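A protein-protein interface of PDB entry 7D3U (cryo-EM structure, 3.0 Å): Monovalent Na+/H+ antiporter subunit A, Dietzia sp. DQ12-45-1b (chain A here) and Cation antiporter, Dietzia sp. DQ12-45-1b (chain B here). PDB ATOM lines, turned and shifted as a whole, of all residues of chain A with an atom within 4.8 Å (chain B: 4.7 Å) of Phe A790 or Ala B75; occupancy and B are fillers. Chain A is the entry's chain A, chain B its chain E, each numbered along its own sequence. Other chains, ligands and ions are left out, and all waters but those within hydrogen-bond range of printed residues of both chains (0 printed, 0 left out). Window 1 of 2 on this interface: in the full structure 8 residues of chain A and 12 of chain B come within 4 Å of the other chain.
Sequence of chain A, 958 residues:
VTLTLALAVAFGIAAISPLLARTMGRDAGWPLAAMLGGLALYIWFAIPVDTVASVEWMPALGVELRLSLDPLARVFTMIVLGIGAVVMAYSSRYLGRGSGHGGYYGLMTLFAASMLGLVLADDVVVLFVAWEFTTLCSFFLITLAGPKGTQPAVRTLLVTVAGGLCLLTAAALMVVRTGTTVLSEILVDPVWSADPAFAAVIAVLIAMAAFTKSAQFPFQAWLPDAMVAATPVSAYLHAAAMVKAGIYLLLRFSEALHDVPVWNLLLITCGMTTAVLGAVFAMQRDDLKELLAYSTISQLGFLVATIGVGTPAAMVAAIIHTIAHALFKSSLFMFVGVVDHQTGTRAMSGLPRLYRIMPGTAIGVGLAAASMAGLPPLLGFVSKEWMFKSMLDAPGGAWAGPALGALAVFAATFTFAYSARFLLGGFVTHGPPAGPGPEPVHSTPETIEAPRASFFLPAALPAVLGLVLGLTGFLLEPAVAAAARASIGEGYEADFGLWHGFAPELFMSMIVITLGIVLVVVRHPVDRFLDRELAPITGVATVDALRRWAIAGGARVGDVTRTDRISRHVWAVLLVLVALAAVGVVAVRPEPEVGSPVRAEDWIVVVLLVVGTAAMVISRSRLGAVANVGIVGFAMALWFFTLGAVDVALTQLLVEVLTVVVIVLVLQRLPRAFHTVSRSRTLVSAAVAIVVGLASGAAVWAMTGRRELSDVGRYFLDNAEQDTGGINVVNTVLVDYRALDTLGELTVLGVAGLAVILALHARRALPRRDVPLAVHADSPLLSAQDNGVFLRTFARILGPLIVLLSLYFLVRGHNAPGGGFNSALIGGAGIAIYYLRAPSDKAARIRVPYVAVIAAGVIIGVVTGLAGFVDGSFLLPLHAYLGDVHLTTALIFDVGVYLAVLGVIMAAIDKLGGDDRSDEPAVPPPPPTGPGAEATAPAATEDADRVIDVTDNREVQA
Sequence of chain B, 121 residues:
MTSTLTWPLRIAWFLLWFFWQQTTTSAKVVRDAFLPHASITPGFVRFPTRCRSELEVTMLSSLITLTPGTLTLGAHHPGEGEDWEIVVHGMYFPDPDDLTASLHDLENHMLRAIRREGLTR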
ATOM      1  N   ASP A 786      16.071 -24.747  24.042  1.00  0.00           N
ATOM      2  CA  ASP A 786      16.199 -23.855  22.900  1.00  0.00           C
ATOM      3  C   ASP A 786      17.639 -23.471  22.598  1.00  0.00           C
ATOM      4  O   ASP A 786      17.905 -22.936  21.518  1.00  0.00           O
ATOM      5  CB  ASP A 786      15.376 -22.584  23.133  1.00  0.00           C
ATOM      6  CG  ASP A 786      14.023 -22.637  22.461  1.00  0.00           C
ATOM      7  OD1 ASP A 786      13.767 -23.609  21.719  1.00  0.00           O
ATOM      8  OD2 ASP A 786      13.215 -21.709  22.673  1.00  0.00           O
ATOM      9  N   ASN A 787      18.571 -23.732  23.514  1.00  0.00           N
ATOM     10  CA  ASN A 787      19.952 -23.305  23.354  1.00  0.00           C
ATOM     11  C   ASN A 787      20.908 -24.439  23.020  1.00  0.00           C
ATOM     12  O   ASN A 787      22.072 -24.170  22.706  1.00  0.00           O
ATOM     13  CB  ASN A 787      20.437 -22.597  24.624  1.00  0.00           C
ATOM     14  CG  ASN A 787      21.588 -21.658  24.358  1.00  0.00           C
ATOM     15  OD1 ASN A 787      21.848 -21.290  23.215  1.00  0.00           O
ATOM     16  ND2 ASN A 787      22.284 -21.261  25.413  1.00  0.00           N
ATOM     17  N   GLY A 788      20.461 -25.689  23.086  1.00  0.00           N
ATOM     18  CA  GLY A 788      21.294 -26.802  22.686  1.00  0.00           C
ATOM     19  C   GLY A 788      21.044 -27.182  21.243  1.00  0.00           C
ATOM     20  O   GLY A 788      21.292 -28.320  20.837  1.00  0.00           O
ATOM     21  N   VAL A 789      20.543 -26.222  20.462  1.00  0.00           N
ATOM     22  CA  VAL A 789      20.220 -26.480  19.063  1.00  0.00           C
ATOM     23  C   VAL A 789      21.474 -26.804  18.268  1.00  0.00           C
ATOM     24  O   VAL A 789      21.415 -27.528  17.267  1.00  0.00           O
ATOM     25  CB  VAL A 789      19.461 -25.279  18.465  1.00  0.00           C
ATOM     26  CG1 VAL A 789      20.379 -24.081  18.316  1.00  0.00           C
ATOM     27  CG2 VAL A 789      18.851 -25.649  17.130  1.00  0.00           C
ATOM     28  N   PHE A 790      22.627 -26.288  18.695  1.00  0.00           N
ATOM     29  CA  PHE A 790      23.863 -26.540  17.964  1.00  0.00           C
ATOM     30  C   PHE A 790      24.267 -28.002  18.063  1.00  0.00           C
ATOM     31  O   PHE A 790      24.606 -28.633  17.055  1.00  0.00           O
ATOM     32  CB  PHE A 790      24.973 -25.632  18.486  1.00  0.00           C
ATOM     33  CG  PHE A 790      24.559 -24.200  18.632  1.00  0.00           C
ATOM     34  CD1 PHE A 790      24.065 -23.498  17.551  1.00  0.00           C
ATOM     35  CD2 PHE A 790      24.670 -23.553  19.847  1.00  0.00           C
ATOM     36  CE1 PHE A 790      23.684 -22.181  17.680  1.00  0.00           C
ATOM     37  CE2 PHE A 790      24.292 -22.236  19.981  1.00  0.00           C
ATOM     38  CZ  PHE A 790      23.799 -21.551  18.895  1.00  0.00           C
ATOM     39  N   LEU A 791      24.235 -28.564  19.270  1.00  0.00           N
ATOM     40  CA  LEU A 791      24.577 -29.971  19.425  1.00  0.00           C
ATOM     41  C   LEU A 791      23.461 -30.887  18.947  1.00  0.00           C
ATOM     42  O   LEU A 791      23.741 -31.964  18.412  1.00  0.00           O
ATOM     43  CB  LEU A 791      24.921 -30.278  20.881  1.00  0.00           C
ATOM     44  CG  LEU A 791      25.551 -31.652  21.103  1.00  0.00           C
ATOM     45  CD1 LEU A 791      26.700 -31.867  20.139  1.00  0.00           C
ATOM     46  CD2 LEU A 791      26.020 -31.801  22.537  1.00  0.00           C
ATOM     47  N   ARG A 792      22.199 -30.486  19.121  1.00  0.00           N
ATOM     48  CA  ARG A 792      21.095 -31.329  18.682  1.00  0.00           C
ATOM     49  C   ARG A 792      21.048 -31.478  17.169  1.00  0.00           C
ATOM     50  O   ARG A 792      20.414 -32.413  16.670  1.00  0.00           O
ATOM     51  CB  ARG A 792      19.765 -30.772  19.193  1.00  0.00           C
ATOM     52  CG  ARG A 792      19.504 -31.064  20.661  1.00  0.00           C
ATOM     53  CD  ARG A 792      18.057 -30.804  21.045  1.00  0.00           C
ATOM     54  NE  ARG A 792      17.754 -29.380  21.139  1.00  0.00           N
ATOM     55  CZ  ARG A 792      17.161 -28.679  20.179  1.00  0.00           C
ATOM     56  NH1 ARG A 792      16.804 -29.272  19.050  1.00  0.00           N
ATOM     57  NH2 ARG A 792      16.922 -27.387  20.350  1.00  0.00           N
ATOM     58  N   THR A 793      21.697 -30.581  16.428  1.00  0.00           N
ATOM     59  CA  THR A 793      21.768 -30.686  14.976  1.00  0.00           C
ATOM     60  C   THR A 793      23.051 -31.358  14.507  1.00  0.00           C
ATOM     61  O   THR A 793      23.011 -32.221  13.627  1.00  0.00           O
ATOM     62  CB  THR A 793      21.643 -29.302  14.333  1.00  0.00           C
ATOM     63  OG1 THR A 793      20.333 -28.781  14.577  1.00  0.00           O
ATOM     64  CG2 THR A 793      21.861 -29.402  12.833  1.00  0.00           C
ATOM     65  N   PHE A 794      24.196 -30.974  15.074  1.00  0.00           N
ATOM     66  CA  PHE A 794      25.442 -31.648  14.726  1.00  0.00           C
ATOM     67  C   PHE A 794      25.385 -33.128  15.064  1.00  0.00           C
ATOM     68  O   PHE A 794      26.053 -33.940  14.416  1.00  0.00           O
ATOM     69  CB  PHE A 794      26.617 -30.989  15.441  1.00  0.00           C
ATOM     70  CG  PHE A 794      27.958 -31.472  14.975  1.00  0.00           C
ATOM     71  CD1 PHE A 794      28.205 -31.678  13.631  1.00  0.00           C
ATOM     72  CD2 PHE A 794      28.976 -31.716  15.881  1.00  0.00           C
ATOM     73  CE1 PHE A 794      29.439 -32.122  13.198  1.00  0.00           C
ATOM     74  CE2 PHE A 794      30.212 -32.159  15.454  1.00  0.00           C
ATOM     75  CZ  PHE A 794      30.443 -32.361  14.111  1.00  0.00           C
ATOM     76  N   VAL B  57      19.960 -22.239  11.467  1.00  0.00           N
ATOM     77  CA  VAL B  57      20.453 -21.337  12.500  1.00  0.00           C
ATOM     78  C   VAL B  57      21.765 -21.847  13.087  1.00  0.00           C
ATOM     79  O   VAL B  57      22.673 -21.059  13.374  1.00  0.00           O
ATOM     80  CB  VAL B  57      19.385 -21.117  13.587  1.00  0.00           C
ATOM     81  CG1 VAL B  57      18.854 -22.436  14.097  1.00  0.00           C
ATOM     82  CG2 VAL B  57      19.951 -20.293  14.728  1.00  0.00           C
ATOM     83  N   THR B  58      21.910 -23.164  13.253  1.00  0.00           N
ATOM     84  CA  THR B  58      23.158 -23.664  13.823  1.00  0.00           C
ATOM     85  C   THR B  58      24.306 -23.526  12.835  1.00  0.00           C
ATOM     86  O   THR B  58      25.438 -23.230  13.234  1.00  0.00           O
ATOM     87  CB  THR B  58      23.028 -25.117  14.278  1.00  0.00           C
ATOM     88  OG1 THR B  58      24.310 -25.587  14.705  1.00  0.00           O
ATOM     89  CG2 THR B  58      22.579 -25.988  13.145  1.00  0.00           C
ATOM     90  N   SER B  61      25.297 -19.926  12.937  1.00  0.00           N
ATOM     91  CA  SER B  61      26.104 -19.653  14.121  1.00  0.00           C
ATOM     92  C   SER B  61      27.520 -20.186  13.962  1.00  0.00           C
ATOM     93  O   SER B  61      28.486 -19.525  14.360  1.00  0.00           O
ATOM     94  CB  SER B  61      25.440 -20.259  15.354  1.00  0.00           C
ATOM     95  OG  SER B  61      26.398 -20.548  16.356  1.00  0.00           O
ATOM     96  N   THR B  72      29.382 -16.758  18.196  1.00  0.00           N
ATOM     97  CA  THR B  72      27.986 -16.900  18.587  1.00  0.00           C
ATOM     98  C   THR B  72      27.912 -17.597  19.938  1.00  0.00           C
ATOM     99  O   THR B  72      28.297 -18.762  20.060  1.00  0.00           O
ATOM    100  CB  THR B  72      27.198 -17.690  17.548  1.00  0.00           C
ATOM    101  OG1 THR B  72      27.280 -17.031  16.281  1.00  0.00           O
ATOM    102  CG2 THR B  72      25.745 -17.789  17.964  1.00  0.00           C
ATOM    103  N   LEU B  73      27.410 -16.886  20.945  1.00  0.00           N
ATOM    104  CA  LEU B  73      27.348 -17.455  22.285  1.00  0.00           C
ATOM    105  C   LEU B  73      26.229 -18.483  22.400  1.00  0.00           C
ATOM    106  O   LEU B  73      26.458 -19.611  22.846  1.00  0.00           O
ATOM    107  CB  LEU B  73      27.173 -16.343  23.318  1.00  0.00           C
ATOM    108  CG  LEU B  73      28.460 -15.868  23.993  1.00  0.00           C
ATOM    109  CD1 LEU B  73      29.428 -15.320  22.969  1.00  0.00           C
ATOM    110  CD2 LEU B  73      28.152 -14.819  25.033  1.00  0.00           C
ATOM    111  N   GLY B  74      25.017 -18.115  22.000  1.00  0.00           N
ATOM    112  CA  GLY B  74      23.906 -19.040  22.094  1.00  0.00           C
ATOM    113  C   GLY B  74      22.765 -18.607  21.202  1.00  0.00           C
ATOM    114  O   GLY B  74      22.830 -17.584  20.519  1.00  0.00           O
ATOM    115  N   ALA B  75      21.708 -19.416  21.214  1.00  0.00           N
ATOM    116  CA  ALA B  75      20.541 -19.173  20.385  1.00  0.00           C
ATOM    117  C   ALA B  75      19.277 -19.424  21.192  1.00  0.00           C
ATOM    118  O   ALA B  75      19.238 -20.298  22.062  1.00  0.00           O
ATOM    119  CB  ALA B  75      20.544 -20.056  19.134  1.00  0.00           C
ATOM    120  N   HIS B  76      18.246 -18.645  20.886  1.00  0.00           N
ATOM    121  CA  HIS B  76      16.928 -18.750  21.496  1.00  0.00           C
ATOM    122  C   HIS B  76      15.988 -17.835  20.734  1.00  0.00           C
ATOM    123  O   HIS B  76      16.423 -16.844  20.141  1.00  0.00           O
ATOM    124  CB  HIS B  76      16.950 -18.363  22.978  1.00  0.00           C
ATOM    125  CG  HIS B  76      16.412 -16.994  23.248  1.00  0.00           C
ATOM    126  ND1 HIS B  76      17.054 -15.846  22.834  1.00  0.00           N
ATOM    127  CD2 HIS B  76      15.288 -16.587  23.885  1.00  0.00           C
ATOM    128  CE1 HIS B  76      16.350 -14.792  23.208  1.00  0.00           C
ATOM    129  NE2 HIS B  76      15.274 -15.214  23.847  1.00  0.00           N
ATOM    130  N   TRP B  84      14.082 -17.476  15.247  1.00  0.00           N
ATOM    131  CA  TRP B  84      15.394 -17.655  15.855  1.00  0.00           C
ATOM    132  C   TRP B  84      16.195 -16.382  16.098  1.00  0.00           C
ATOM    133  O   TRP B  84      16.364 -15.551  15.202  1.00  0.00           O
ATOM    134  CB  TRP B  84      16.304 -18.724  15.253  1.00  0.00           C
ATOM    135  CG  TRP B  84      15.817 -20.117  15.443  1.00  0.00           C
ATOM    136  CD1 TRP B  84      14.937 -20.793  14.655  1.00  0.00           C
ATOM    137  CD2 TRP B  84      16.186 -21.015  16.495  1.00  0.00           C
ATOM    138  NE1 TRP B  84      14.733 -22.058  15.149  1.00  0.00           N
ATOM    139  CE2 TRP B  84      15.490 -22.218  16.279  1.00  0.00           C
ATOM    140  CE3 TRP B  84      17.037 -20.917  17.597  1.00  0.00           C
ATOM    141  CZ2 TRP B  84      15.619 -23.314  17.125  1.00  0.00           C
ATOM    142  CZ3 TRP B  84      17.163 -22.005  18.435  1.00  0.00           C
ATOM    143  CH2 TRP B  84      16.458 -23.188  18.196  1.00  0.00           C
ATOM    144  N   GLU B  85      16.684 -16.235  17.324  1.00  0.00           N
ATOM    145  CA  GLU B  85      17.597 -15.167  17.697  1.00  0.00           C
ATOM    146  C   GLU B  85      18.914 -15.771  18.160  1.00  0.00           C
ATOM    147  O   GLU B  85      18.945 -16.857  18.741  1.00  0.00           O
ATOM    148  CB  GLU B  85      17.012 -14.299  18.815  1.00  0.00           C
ATOM    149  CG  GLU B  85      16.278 -13.064  18.338  1.00  0.00           C
ATOM    150  CD  GLU B  85      16.116 -12.033  19.436  1.00  0.00           C
ATOM    151  OE1 GLU B  85      16.675 -12.241  20.532  1.00  0.00           O
ATOM    152  OE2 GLU B  85      15.433 -11.013  19.204  1.00  0.00           O
ATOM    153  N   ILE B  86      20.008 -15.064  17.893  1.00  0.00           N
ATOM    154  CA  ILE B  86      21.319 -15.500  18.347  1.00  0.00           C
ATOM    155  C   ILE B  86      21.969 -14.374  19.138  1.00  0.00           C
ATOM    156  O   ILE B  86      21.575 -13.210  19.053  1.00  0.00           O
ATOM    157  CB  ILE B  86      22.230 -15.946  17.186  1.00  0.00           C
ATOM    158  CG1 ILE B  86      22.357 -14.838  16.145  1.00  0.00           C
ATOM    159  CG2 ILE B  86      21.698 -17.217  16.552  1.00  0.00           C
ATOM    160  CD1 ILE B  86      23.075 -15.275  14.893  1.00  0.00           C
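The side-chain amide oxygen (OD1) of Asn A787 is in hydrogen-bond range of the backbone NH (N) of Ala B75 (2.7 Å). O of Asp A786 lies close to O of Ala B75 (3.0 Å).
The side-chain hydroxyl of Thr B72 lies within hydrogen-bond range of the backbone carbonyl oxygen of Ser B61 (3.4 Å). The backbone carbonyl oxygen (O) of Val A789 sits at hydrogen-bond distance from the side-chain hydroxyl (OG1) of Thr A793, 3.2 Å away.
Trp B84 touches Asp A786. Gly B74 touches Asn A787 (CA to OD1, 3.2 Å). Trp B84 touches Val A789 (CH2 to CG2, 3.6 Å). Thr B58 touches Phe A790. Phe A790 touches Ser B61 (CE1 to OG, 3.4 Å). Gly B74 touches Phe A790 (CA to CE2, 3.9 Å). Ala B75 touches Phe A790 (CB to CZ, 3.6 Å). Thr B58 touches Thr A793.
Phe A790 touches just these residues of chain B: Thr B58, Ser B61, Gly B74 and Ala B75. Ala B75 touches just these residues of chain A: Asp A786, Asn A787 and Phe A790. Of the printed residues of chain B, Thr A793 touches Thr B58 (3.5 Å). Of the printed residues of chain A, Trp B84 touches Asp A786 (3.3 Å) and Val A789 (3.6 Å). The nearest residue of chain A that does not touch Ala B75 is Val A789 (4.1 Å). The nearest printed residue of chain A that does not touch Trp B84 is Arg A792 (4.7 Å).
Printed residues of chain B that touch a printed residue of chain A: Thr B58, Ser B61, Gly B74, Ala B75 and Trp B84. Of the 9 printed residues of chain A, 5 touch a printed residue of chain B. Printed residues of chain A that touch a printed residue of chain B: Asp A786, Asn A787, Val A789, Phe A790 and Thr A793. Hydrophobic or aromatic side chains of chain A within 4 Å of the printed part of chain B: Val A789 and Phe A790. Among the printed residues, no Asp or Glu carboxylate lies within 4 Å of a Lys or Arg side-chain nitrogen of the other chain.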
